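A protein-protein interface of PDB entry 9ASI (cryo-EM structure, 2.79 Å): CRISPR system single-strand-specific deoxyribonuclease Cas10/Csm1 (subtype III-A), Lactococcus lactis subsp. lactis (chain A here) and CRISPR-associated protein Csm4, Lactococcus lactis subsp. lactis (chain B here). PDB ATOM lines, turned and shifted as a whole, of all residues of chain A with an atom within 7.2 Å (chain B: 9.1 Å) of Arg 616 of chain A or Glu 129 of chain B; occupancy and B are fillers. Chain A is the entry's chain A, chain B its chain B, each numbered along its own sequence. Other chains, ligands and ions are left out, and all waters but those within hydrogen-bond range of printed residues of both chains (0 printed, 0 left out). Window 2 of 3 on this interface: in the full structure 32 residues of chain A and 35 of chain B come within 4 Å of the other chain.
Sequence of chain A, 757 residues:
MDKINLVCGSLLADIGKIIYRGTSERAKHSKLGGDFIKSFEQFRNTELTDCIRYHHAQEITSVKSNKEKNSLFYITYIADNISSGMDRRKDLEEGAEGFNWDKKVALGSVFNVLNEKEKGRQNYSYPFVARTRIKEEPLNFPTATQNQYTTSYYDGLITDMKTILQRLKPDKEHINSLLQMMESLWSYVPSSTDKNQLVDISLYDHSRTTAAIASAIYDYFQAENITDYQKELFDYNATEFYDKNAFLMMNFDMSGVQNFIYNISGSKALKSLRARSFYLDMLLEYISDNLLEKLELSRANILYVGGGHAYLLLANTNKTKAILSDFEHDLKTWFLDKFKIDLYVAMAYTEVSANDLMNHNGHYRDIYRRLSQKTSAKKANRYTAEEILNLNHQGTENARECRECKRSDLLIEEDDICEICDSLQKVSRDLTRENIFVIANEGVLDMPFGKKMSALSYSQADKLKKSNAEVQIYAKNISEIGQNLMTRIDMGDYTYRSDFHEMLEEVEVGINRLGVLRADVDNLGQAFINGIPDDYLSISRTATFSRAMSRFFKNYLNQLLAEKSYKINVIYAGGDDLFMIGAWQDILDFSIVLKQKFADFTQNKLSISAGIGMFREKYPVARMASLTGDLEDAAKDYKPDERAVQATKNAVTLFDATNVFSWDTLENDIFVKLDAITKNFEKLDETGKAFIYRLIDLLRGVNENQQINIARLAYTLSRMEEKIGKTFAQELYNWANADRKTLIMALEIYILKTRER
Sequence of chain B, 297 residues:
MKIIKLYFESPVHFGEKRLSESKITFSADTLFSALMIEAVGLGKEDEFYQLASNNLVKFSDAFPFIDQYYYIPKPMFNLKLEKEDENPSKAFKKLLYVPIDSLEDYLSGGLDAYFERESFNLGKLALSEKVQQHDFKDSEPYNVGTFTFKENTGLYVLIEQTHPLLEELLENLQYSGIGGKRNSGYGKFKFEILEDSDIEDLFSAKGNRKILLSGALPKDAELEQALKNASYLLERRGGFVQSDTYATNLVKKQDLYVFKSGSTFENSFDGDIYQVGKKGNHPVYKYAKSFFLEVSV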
ATOM      1  N   LEU A 270      10.243  34.849 -20.210  1.00  0.00           N
ATOM      2  CA  LEU A 270       9.224  35.845 -19.891  1.00  0.00           C
ATOM      3  C   LEU A 270       9.774  36.948 -18.997  1.00  0.00           C
ATOM      4  O   LEU A 270       9.302  38.089 -19.058  1.00  0.00           O
ATOM      5  CB  LEU A 270       8.026  35.170 -19.223  1.00  0.00           C
ATOM      6  CG  LEU A 270       6.979  34.544 -20.146  1.00  0.00           C
ATOM      7  CD1 LEU A 270       6.119  33.546 -19.384  1.00  0.00           C
ATOM      8  CD2 LEU A 270       6.116  35.618 -20.785  1.00  0.00           C
ATOM      9  N   LEU A 504       0.290  35.178 -11.477  1.00  0.00           N
ATOM     10  CA  LEU A 504      -0.914  34.534 -11.990  1.00  0.00           C
ATOM     11  C   LEU A 504      -1.745  33.905 -10.878  1.00  0.00           C
ATOM     12  O   LEU A 504      -2.978  33.940 -10.932  1.00  0.00           O
ATOM     13  CB  LEU A 504      -0.538  33.478 -13.031  1.00  0.00           C
ATOM     14  CG  LEU A 504      -0.577  33.920 -14.495  1.00  0.00           C
ATOM     15  CD1 LEU A 504      -0.210  32.764 -15.410  1.00  0.00           C
ATOM     16  CD2 LEU A 504      -1.946  34.477 -14.854  1.00  0.00           C
ATOM     17  N   ASN A 512      -6.354  29.796 -15.532  1.00  0.00           N
ATOM     18  CA  ASN A 512      -4.894  29.765 -15.437  1.00  0.00           C
ATOM     19  C   ASN A 512      -4.241  30.029 -16.790  1.00  0.00           C
ATOM     20  O   ASN A 512      -3.399  29.264 -17.260  1.00  0.00           O
ATOM     21  CB  ASN A 512      -4.438  28.431 -14.860  1.00  0.00           C
ATOM     22  CG  ASN A 512      -3.047  28.499 -14.258  1.00  0.00           C
ATOM     23  OD1 ASN A 512      -2.373  29.526 -14.336  1.00  0.00           O
ATOM     24  ND2 ASN A 512      -2.611  27.403 -13.651  1.00  0.00           N
ATOM     25  N   ARG A 513      -4.631  31.129 -17.428  1.00  0.00           N
ATOM     26  CA  ARG A 513      -4.101  31.519 -18.723  1.00  0.00           C
ATOM     27  C   ARG A 513      -3.383  32.857 -18.605  1.00  0.00           C
ATOM     28  O   ARG A 513      -3.680  33.672 -17.728  1.00  0.00           O
ATOM     29  CB  ARG A 513      -5.211  31.615 -19.778  1.00  0.00           C
ATOM     30  CG  ARG A 513      -5.330  30.398 -20.683  1.00  0.00           C
ATOM     31  CD  ARG A 513      -5.326  29.097 -19.895  1.00  0.00           C
ATOM     32  NE  ARG A 513      -5.189  27.933 -20.762  1.00  0.00           N
ATOM     33  CZ  ARG A 513      -4.739  26.752 -20.363  1.00  0.00           C
ATOM     34  NH1 ARG A 513      -4.369  26.539 -19.111  1.00  0.00           N
ATOM     35  NH2 ARG A 513      -4.658  25.758 -21.244  1.00  0.00           N
ATOM     36  N   LEU A 514      -2.429  33.072 -19.503  1.00  0.00           N
ATOM     37  CA  LEU A 514      -1.635  34.294 -19.536  1.00  0.00           C
ATOM     38  C   LEU A 514      -2.131  35.167 -20.680  1.00  0.00           C
ATOM     39  O   LEU A 514      -2.010  34.790 -21.851  1.00  0.00           O
ATOM     40  CB  LEU A 514      -0.150  33.974 -19.700  1.00  0.00           C
ATOM     41  CG  LEU A 514       0.821  35.126 -19.448  1.00  0.00           C
ATOM     42  CD1 LEU A 514       0.691  35.628 -18.019  1.00  0.00           C
ATOM     43  CD2 LEU A 514       2.246  34.688 -19.738  1.00  0.00           C
ATOM     44  N   MET A 614      -4.469  33.965 -25.094  1.00  0.00           N
ATOM     45  CA  MET A 614      -4.363  33.147 -23.894  1.00  0.00           C
ATOM     46  C   MET A 614      -3.241  32.136 -24.080  1.00  0.00           C
ATOM     47  O   MET A 614      -3.197  31.430 -25.093  1.00  0.00           O
ATOM     48  CB  MET A 614      -5.675  32.424 -23.595  1.00  0.00           C
ATOM     49  CG  MET A 614      -6.906  33.308 -23.602  1.00  0.00           C
ATOM     50  SD  MET A 614      -8.402  32.360 -23.261  1.00  0.00           S
ATOM     51  CE  MET A 614      -8.994  32.030 -24.918  1.00  0.00           C
ATOM     52  N   PHE A 615      -2.340  32.069 -23.104  1.00  0.00           N
ATOM     53  CA  PHE A 615      -1.181  31.196 -23.187  1.00  0.00           C
ATOM     54  C   PHE A 615      -0.976  30.496 -21.853  1.00  0.00           C
ATOM     55  O   PHE A 615      -1.386  30.993 -20.801  1.00  0.00           O
ATOM     56  CB  PHE A 615       0.083  31.976 -23.574  1.00  0.00           C
ATOM     57  CG  PHE A 615      -0.095  32.855 -24.779  1.00  0.00           C
ATOM     58  CD1 PHE A 615      -0.354  32.302 -26.025  1.00  0.00           C
ATOM     59  CD2 PHE A 615      -0.014  34.233 -24.667  1.00  0.00           C
ATOM     60  CE1 PHE A 615      -0.521  33.107 -27.135  1.00  0.00           C
ATOM     61  CE2 PHE A 615      -0.179  35.043 -25.774  1.00  0.00           C
ATOM     62  CZ  PHE A 615      -0.434  34.479 -27.010  1.00  0.00           C
ATOM     63  N   ARG A 616      -0.332  29.334 -21.910  1.00  0.00           N
ATOM     64  CA  ARG A 616      -0.029  28.573 -20.711  1.00  0.00           C
ATOM     65  C   ARG A 616       1.099  29.251 -19.936  1.00  0.00           C
ATOM     66  O   ARG A 616       1.588  30.326 -20.297  1.00  0.00           O
ATOM     67  CB  ARG A 616       0.343  27.138 -21.078  1.00  0.00           C
ATOM     68  CG  ARG A 616      -0.766  26.366 -21.771  1.00  0.00           C
ATOM     69  CD  ARG A 616      -0.318  24.961 -22.144  1.00  0.00           C
ATOM     70  NE  ARG A 616      -0.100  24.123 -20.970  1.00  0.00           N
ATOM     71  CZ  ARG A 616       1.086  23.688 -20.569  1.00  0.00           C
ATOM     72  NH1 ARG A 616       2.193  23.988 -21.229  1.00  0.00           N
ATOM     73  NH2 ARG A 616       1.165  22.931 -19.479  1.00  0.00           N
ATOM     74  N   GLU A 617       1.523  28.608 -18.848  1.00  0.00           N
ATOM     75  CA  GLU A 617       2.615  29.139 -18.047  1.00  0.00           C
ATOM     76  C   GLU A 617       3.982  28.869 -18.661  1.00  0.00           C
ATOM     77  O   GLU A 617       4.970  29.466 -18.220  1.00  0.00           O
ATOM     78  CB  GLU A 617       2.563  28.562 -16.630  1.00  0.00           C
ATOM     79  CG  GLU A 617       2.255  27.076 -16.566  1.00  0.00           C
ATOM     80  CD  GLU A 617       1.887  26.620 -15.167  1.00  0.00           C
ATOM     81  OE1 GLU A 617       1.871  27.468 -14.250  1.00  0.00           O
ATOM     82  OE2 GLU A 617       1.617  25.416 -14.982  1.00  0.00           O
ATOM     83  N   LYS A 618       4.064  27.991 -19.665  1.00  0.00           N
ATOM     84  CA  LYS A 618       5.332  27.684 -20.315  1.00  0.00           C
ATOM     85  C   LYS A 618       5.220  27.762 -21.836  1.00  0.00           C
ATOM     86  O   LYS A 618       6.020  27.145 -22.547  1.00  0.00           O
ATOM     87  CB  LYS A 618       5.834  26.306 -19.877  1.00  0.00           C
ATOM     88  CG  LYS A 618       7.338  26.125 -19.991  1.00  0.00           C
ATOM     89  CD  LYS A 618       8.081  26.994 -18.992  1.00  0.00           C
ATOM     90  CE  LYS A 618       7.987  26.426 -17.586  1.00  0.00           C
ATOM     91  NZ  LYS A 618       8.824  27.192 -16.620  1.00  0.00           N
ATOM     92  N   TYR A 619       4.243  28.504 -22.346  1.00  0.00           N
ATOM     93  CA  TYR A 619       4.116  28.698 -23.779  1.00  0.00           C
ATOM     94  C   TYR A 619       5.316  29.485 -24.307  1.00  0.00           C
ATOM     95  O   TYR A 619       5.860  30.344 -23.608  1.00  0.00           O
ATOM     96  CB  TYR A 619       2.820  29.441 -24.093  1.00  0.00           C
ATOM     97  CG  TYR A 619       2.235  29.174 -25.460  1.00  0.00           C
ATOM     98  CD1 TYR A 619       1.586  27.979 -25.739  1.00  0.00           C
ATOM     99  CD2 TYR A 619       2.304  30.131 -26.464  1.00  0.00           C
ATOM    100  CE1 TYR A 619       1.039  27.735 -26.985  1.00  0.00           C
ATOM    101  CE2 TYR A 619       1.758  29.899 -27.711  1.00  0.00           C
ATOM    102  CZ  TYR A 619       1.128  28.699 -27.966  1.00  0.00           C
ATOM    103  OH  TYR A 619       0.584  28.460 -29.206  1.00  0.00           O
ATOM    104  N   PRO A 620       5.766  29.193 -25.528  1.00  0.00           N
ATOM    105  CA  PRO A 620       6.904  29.934 -26.094  1.00  0.00           C
ATOM    106  C   PRO A 620       6.578  31.413 -26.232  1.00  0.00           C
ATOM    107  O   PRO A 620       5.610  31.795 -26.892  1.00  0.00           O
ATOM    108  CB  PRO A 620       7.112  29.267 -27.458  1.00  0.00           C
ATOM    109  CG  PRO A 620       6.551  27.901 -27.289  1.00  0.00           C
ATOM    110  CD  PRO A 620       5.355  28.081 -26.401  1.00  0.00           C
ATOM    111  N   ARG A 623       6.530  32.572 -29.681  1.00  0.00           N
ATOM    112  CA  ARG A 623       5.256  32.182 -30.271  1.00  0.00           C
ATOM    113  C   ARG A 623       4.119  33.035 -29.725  1.00  0.00           C
ATOM    114  O   ARG A 623       3.202  33.400 -30.468  1.00  0.00           O
ATOM    115  CB  ARG A 623       4.998  30.694 -30.025  1.00  0.00           C
ATOM    116  CG  ARG A 623       3.747  30.160 -30.701  1.00  0.00           C
ATOM    117  CD  ARG A 623       3.551  28.670 -30.448  1.00  0.00           C
ATOM    118  NE  ARG A 623       4.322  27.831 -31.358  1.00  0.00           N
ATOM    119  CZ  ARG A 623       4.198  26.513 -31.443  1.00  0.00           C
ATOM    120  NH1 ARG A 623       3.336  25.849 -30.694  1.00  0.00           N
ATOM    121  NH2 ARG A 623       4.958  25.845 -32.304  1.00  0.00           N
ATOM    122  N   MET A 624       4.168  33.372 -28.431  1.00  0.00           N
ATOM    123  CA  MET A 624       3.195  34.303 -27.866  1.00  0.00           C
ATOM    124  C   MET A 624       3.173  35.604 -28.654  1.00  0.00           C
ATOM    125  O   MET A 624       2.112  36.075 -29.078  1.00  0.00           O
ATOM    126  CB  MET A 624       3.522  34.602 -26.401  1.00  0.00           C
ATOM    127  CG  MET A 624       3.314  33.474 -25.413  1.00  0.00           C
ATOM    128  SD  MET A 624       3.534  34.105 -23.732  1.00  0.00           S
ATOM    129  CE  MET A 624       3.699  32.596 -22.784  1.00  0.00           C
ATOM    130  N   SER B  20       9.863  25.862 -32.428  1.00  0.00           N
ATOM    131  CA  SER B  20       8.521  26.290 -32.058  1.00  0.00           C
ATOM    132  C   SER B  20       7.832  27.091 -33.152  1.00  0.00           C
ATOM    133  O   SER B  20       6.614  27.275 -33.089  1.00  0.00           O
ATOM    134  CB  SER B  20       8.565  27.108 -30.769  1.00  0.00           C
ATOM    135  OG  SER B  20       9.234  28.341 -30.963  1.00  0.00           O
ATOM    136  N   ALA B 126       0.439  26.196 -37.352  1.00  0.00           N
ATOM    137  CA  ALA B 126      -0.186  25.384 -36.324  1.00  0.00           C
ATOM    138  C   ALA B 126       0.787  25.107 -35.191  1.00  0.00           C
ATOM    139  O   ALA B 126       1.998  25.000 -35.396  1.00  0.00           O
ATOM    140  CB  ALA B 126      -0.691  24.059 -36.896  1.00  0.00           C
ATOM    141  N   LEU B 127       0.237  25.010 -33.988  1.00  0.00           N
ATOM    142  CA  LEU B 127       0.960  24.466 -32.853  1.00  0.00           C
ATOM    143  C   LEU B 127       0.849  22.949 -32.861  1.00  0.00           C
ATOM    144  O   LEU B 127      -0.163  22.381 -33.282  1.00  0.00           O
ATOM    145  CB  LEU B 127       0.409  25.017 -31.534  1.00  0.00           C
ATOM    146  CG  LEU B 127      -0.947  24.519 -31.011  1.00  0.00           C
ATOM    147  CD1 LEU B 127      -1.123  24.892 -29.547  1.00  0.00           C
ATOM    148  CD2 LEU B 127      -2.114  25.052 -31.831  1.00  0.00           C
ATOM    149  N   SER B 128       1.904  22.288 -32.401  1.00  0.00           N
ATOM    150  CA  SER B 128       1.904  20.829 -32.305  1.00  0.00           C
ATOM    151  C   SER B 128       2.583  20.471 -30.988  1.00  0.00           C
ATOM    152  O   SER B 128       3.800  20.286 -30.938  1.00  0.00           O
ATOM    153  CB  SER B 128       2.600  20.197 -33.496  1.00  0.00           C
ATOM    154  OG  SER B 128       2.726  18.802 -33.319  1.00  0.00           O
ATOM    155  N   GLU B 129       1.788  20.373 -29.929  1.00  0.00           N
ATOM    156  CA  GLU B 129       2.318  20.113 -28.599  1.00  0.00           C
ATOM    157  C   GLU B 129       2.701  18.644 -28.482  1.00  0.00           C
ATOM    158  O   GLU B 129       1.850  17.760 -28.611  1.00  0.00           O
ATOM    159  CB  GLU B 129       1.295  20.502 -27.536  1.00  0.00           C
ATOM    160  CG  GLU B 129       1.296  21.987 -27.213  1.00  0.00           C
ATOM    161  CD  GLU B 129       0.085  22.413 -26.410  1.00  0.00           C
ATOM    162  OE1 GLU B 129      -0.967  22.691 -27.021  1.00  0.00           O
ATOM    163  OE2 GLU B 129       0.184  22.469 -25.166  1.00  0.00           O
ATOM    164  N   LYS B 130       3.981  18.390 -28.230  1.00  0.00           N
ATOM    165  CA  LYS B 130       4.531  17.050 -28.147  1.00  0.00           C
ATOM    166  C   LYS B 130       5.244  16.895 -26.814  1.00  0.00           C
ATOM    167  O   LYS B 130       5.376  17.850 -26.049  1.00  0.00           O
ATOM    168  CB  LYS B 130       5.499  16.781 -29.300  1.00  0.00           C
ATOM    169  CG  LYS B 130       4.976  17.178 -30.653  1.00  0.00           C
ATOM    170  CD  LYS B 130       5.458  16.218 -31.704  1.00  0.00           C
ATOM    171  CE  LYS B 130       4.761  16.468 -33.009  1.00  0.00           C
ATOM    172  NZ  LYS B 130       3.378  15.933 -32.983  1.00  0.00           N
ATOM    173  N   VAL B 131       5.710  15.675 -26.532  1.00  0.00           N
ATOM    174  CA  VAL B 131       6.470  15.393 -25.320  1.00  0.00           C
ATOM    175  C   VAL B 131       7.485  14.297 -25.575  1.00  0.00           C
ATOM    176  O   VAL B 131       7.410  13.564 -26.558  1.00  0.00           O
ATOM    177  CB  VAL B 131       5.593  14.972 -24.119  1.00  0.00           C
ATOM    178  CG1 VAL B 131       4.684  16.057 -23.750  1.00  0.00           C
ATOM    179  CG2 VAL B 131       4.794  13.730 -24.460  1.00  0.00           C
ATOM    180  N   GLN B 132       8.450  14.205 -24.670  1.00  0.00           N
ATOM    181  CA  GLN B 132       9.328  13.053 -24.533  1.00  0.00           C
ATOM    182  C   GLN B 132       8.881  12.327 -23.273  1.00  0.00           C
ATOM    183  O   GLN B 132       9.154  12.776 -22.159  1.00  0.00           O
ATOM    184  CB  GLN B 132      10.788  13.477 -24.444  1.00  0.00           C
ATOM    185  CG  GLN B 132      11.753  12.322 -24.390  1.00  0.00           C
ATOM    186  CD  GLN B 132      13.167  12.773 -24.146  1.00  0.00           C
ATOM    187  OE1 GLN B 132      13.426  13.958 -23.949  1.00  0.00           O
ATOM    188  NE2 GLN B 132      14.098  11.829 -24.158  1.00  0.00           N
ATOM    189  N   GLU B 140       8.839  15.653 -21.002  1.00  0.00           N
ATOM    190  CA  GLU B 140       9.428  16.880 -21.533  1.00  0.00           C
ATOM    191  C   GLU B 140       8.520  17.472 -22.602  1.00  0.00           C
ATOM    192  O   GLU B 140       8.637  17.121 -23.783  1.00  0.00           O
ATOM    193  CB  GLU B 140      10.821  16.606 -22.105  1.00  0.00           C
ATOM    194  CG  GLU B 140      11.952  16.758 -21.106  1.00  0.00           C
ATOM    195  CD  GLU B 140      12.201  15.492 -20.314  1.00  0.00           C
ATOM    196  OE1 GLU B 140      11.291  14.643 -20.249  1.00  0.00           O
ATOM    197  OE2 GLU B 140      13.305  15.342 -19.752  1.00  0.00           O
ATOM    198  N   PRO B 141       7.608  18.379 -22.249  1.00  0.00           N
ATOM    199  CA  PRO B 141       6.726  18.965 -23.264  1.00  0.00           C
ATOM    200  C   PRO B 141       7.487  19.904 -24.188  1.00  0.00           C
ATOM    201  O   PRO B 141       8.183  20.816 -23.737  1.00  0.00           O
ATOM    202  CB  PRO B 141       5.680  19.720 -22.436  1.00  0.00           C
ATOM    203  CG  PRO B 141       5.775  19.146 -21.076  1.00  0.00           C
ATOM    204  CD  PRO B 141       7.205  18.776 -20.893  1.00  0.00           C
ATOM    205  N   TYR B 142       7.342  19.675 -25.489  1.00  0.00           N
ATOM    206  CA  TYR B 142       7.851  20.577 -26.507  1.00  0.00           C
ATOM    207  C   TYR B 142       6.799  20.715 -27.593  1.00  0.00           C
ATOM    208  O   TYR B 142       5.934  19.857 -27.758  1.00  0.00           O
ATOM    209  CB  TYR B 142       9.167  20.084 -27.107  1.00  0.00           C
ATOM    210  CG  TYR B 142       9.030  18.860 -27.980  1.00  0.00           C
ATOM    211  CD1 TYR B 142       8.924  17.596 -27.425  1.00  0.00           C
ATOM    212  CD2 TYR B 142       9.027  18.967 -29.361  1.00  0.00           C
ATOM    213  CE1 TYR B 142       8.809  16.480 -28.216  1.00  0.00           C
ATOM    214  CE2 TYR B 142       8.909  17.856 -30.160  1.00  0.00           C
ATOM    215  CZ  TYR B 142       8.802  16.616 -29.583  1.00  0.00           C
ATOM    216  OH  TYR B 142       8.682  15.506 -30.381  1.00  0.00           O
ATOM    217  N   ASN B 143       6.870  21.810 -28.334  1.00  0.00           N
ATOM    218  CA  ASN B 143       5.966  22.017 -29.450  1.00  0.00           C
ATOM    219  C   ASN B 143       6.764  22.268 -30.718  1.00  0.00           C
ATOM    220  O   ASN B 143       7.868  22.813 -30.684  1.00  0.00           O
ATOM    221  CB  ASN B 143       4.986  23.164 -29.182  1.00  0.00           C
ATOM    222  CG  ASN B 143       5.658  24.386 -28.622  1.00  0.00           C
ATOM    223  OD1 ASN B 143       6.881  24.480 -28.592  1.00  0.00           O
ATOM    224  ND2 ASN B 143       4.858  25.329 -28.151  1.00  0.00           N
ATOM    225  N   VAL B 144       6.195  21.830 -31.835  1.00  0.00           N
ATOM    226  CA  VAL B 144       6.810  21.945 -33.148  1.00  0.00           C
ATOM    227  C   VAL B 144       5.951  22.888 -33.968  1.00  0.00           C
ATOM    228  O   VAL B 144       4.751  22.647 -34.144  1.00  0.00           O
ATOM    229  CB  VAL B 144       6.938  20.578 -33.839  1.00  0.00           C
ATOM    230  CG1 VAL B 144       7.426  20.742 -35.264  1.00  0.00           C
ATOM    231  CG2 VAL B 144       7.859  19.672 -33.054  1.00  0.00           C
ATOM    232  N   GLY B 145       6.555  23.965 -34.459  1.00  0.00           N
ATOM    233  CA  GLY B 145       5.855  24.859 -35.356  1.00  0.00           C
ATOM    234  C   GLY B 145       5.671  24.187 -36.695  1.00  0.00           C
ATOM    235  O   GLY B 145       6.653  23.738 -37.308  1.00  0.00           O
ATOM    236  N   THR B 146       4.431  24.086 -37.158  1.00  0.00           N
ATOM    237  CA  THR B 146       4.117  23.416 -38.409  1.00  0.00           C
ATOM    238  C   THR B 146       3.311  24.357 -39.295  1.00  0.00           C
ATOM    239  O   THR B 146       3.016  25.496 -38.923  1.00  0.00           O
ATOM    240  CB  THR B 146       3.357  22.105 -38.163  1.00  0.00           C
ATOM    241  OG1 THR B 146       2.136  22.378 -37.469  1.00  0.00           O
ATOM    242  CG2 THR B 146       4.197  21.157 -37.333  1.00  0.00           C
ATOM    243  N   TYR B 186       5.783  14.898 -40.616  1.00  0.00           N
ATOM    244  CA  TYR B 186       5.583  16.240 -41.154  1.00  0.00           C
ATOM    245  C   TYR B 186       6.016  16.395 -42.605  1.00  0.00           C
ATOM    246  O   TYR B 186       5.192  16.778 -43.438  1.00  0.00           O
ATOM    247  CB  TYR B 186       6.278  17.255 -40.246  1.00  0.00           C
ATOM    248  CG  TYR B 186       5.511  17.420 -38.965  1.00  0.00           C
ATOM    249  CD1 TYR B 186       4.164  17.734 -38.990  1.00  0.00           C
ATOM    250  CD2 TYR B 186       6.111  17.211 -37.736  1.00  0.00           C
ATOM    251  CE1 TYR B 186       3.445  17.866 -37.833  1.00  0.00           C
ATOM    252  CE2 TYR B 186       5.399  17.344 -36.567  1.00  0.00           C
ATOM    253  CZ  TYR B 186       4.064  17.674 -36.622  1.00  0.00           C
ATOM    254  OH  TYR B 186       3.337  17.811 -35.466  1.00  0.00           O
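The guanidinium group (NH1) of Arg 623 of chain A lies close to the side-chain amide nitrogen (ND2) of Asn 143 of chain B (3.0 Å).
NE of Arg 623 of chain A sits at hydrogen-bond distance from O of Ser 20 of chain B (2.9 Å).
The guanidinium group (NH2) of Arg 623 of chain A sits close to the backbone NH (N) of Gly 145 of chain B.
O of Ser 128 of chain B lies within hydrogen-bond range of N of Val 144 of chain B, at 3.0 Å.
Among the printed residues, merely in contact across the chains: Arg 616 of chain A with Glu 129 of chain B (3.9 Å), Tyr 619 of chain A with Leu 127 of chain B (3.97 Å), Pro 620 of chain A with Asn 143 of chain B (3.2 Å), Arg 623 of chain A with Leu 127 of chain B (3.2 Å) and Arg 623 of chain A with Val 144 of chain B (3.5 Å).
Of chain B, only Glu 129 comes within 4 Å of Arg 616 of chain A.
Printed residues of chain B within 4 Å of Arg 623 of chain A: Ser 20, Leu 127, Asn 143, Val 144 and Gly 145.
Of the printed residues of chain A, Glu 129 of chain B touches Arg 616 (3.9 Å).
Printed residues of chain A within 4 Å of Val 144 of chain B: Arg 623.
The nearest residue of chain B that does not touch Arg 616 of chain A is Pro 141 of chain B (5.6 Å).
Hydrophobic or aromatic side chains of chain A that line the printed part of chain B: Tyr 619 and Pro 620.
Hydrophobic or aromatic side chains of chain B that line the printed part of chain A: Leu 127.
Among the printed residues, 8 pairs touch across the chains.
Among the printed residues, no Asp or Glu carboxylate lies within 4 Å of a Lys or Arg side-chain nitrogen of the other chain.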
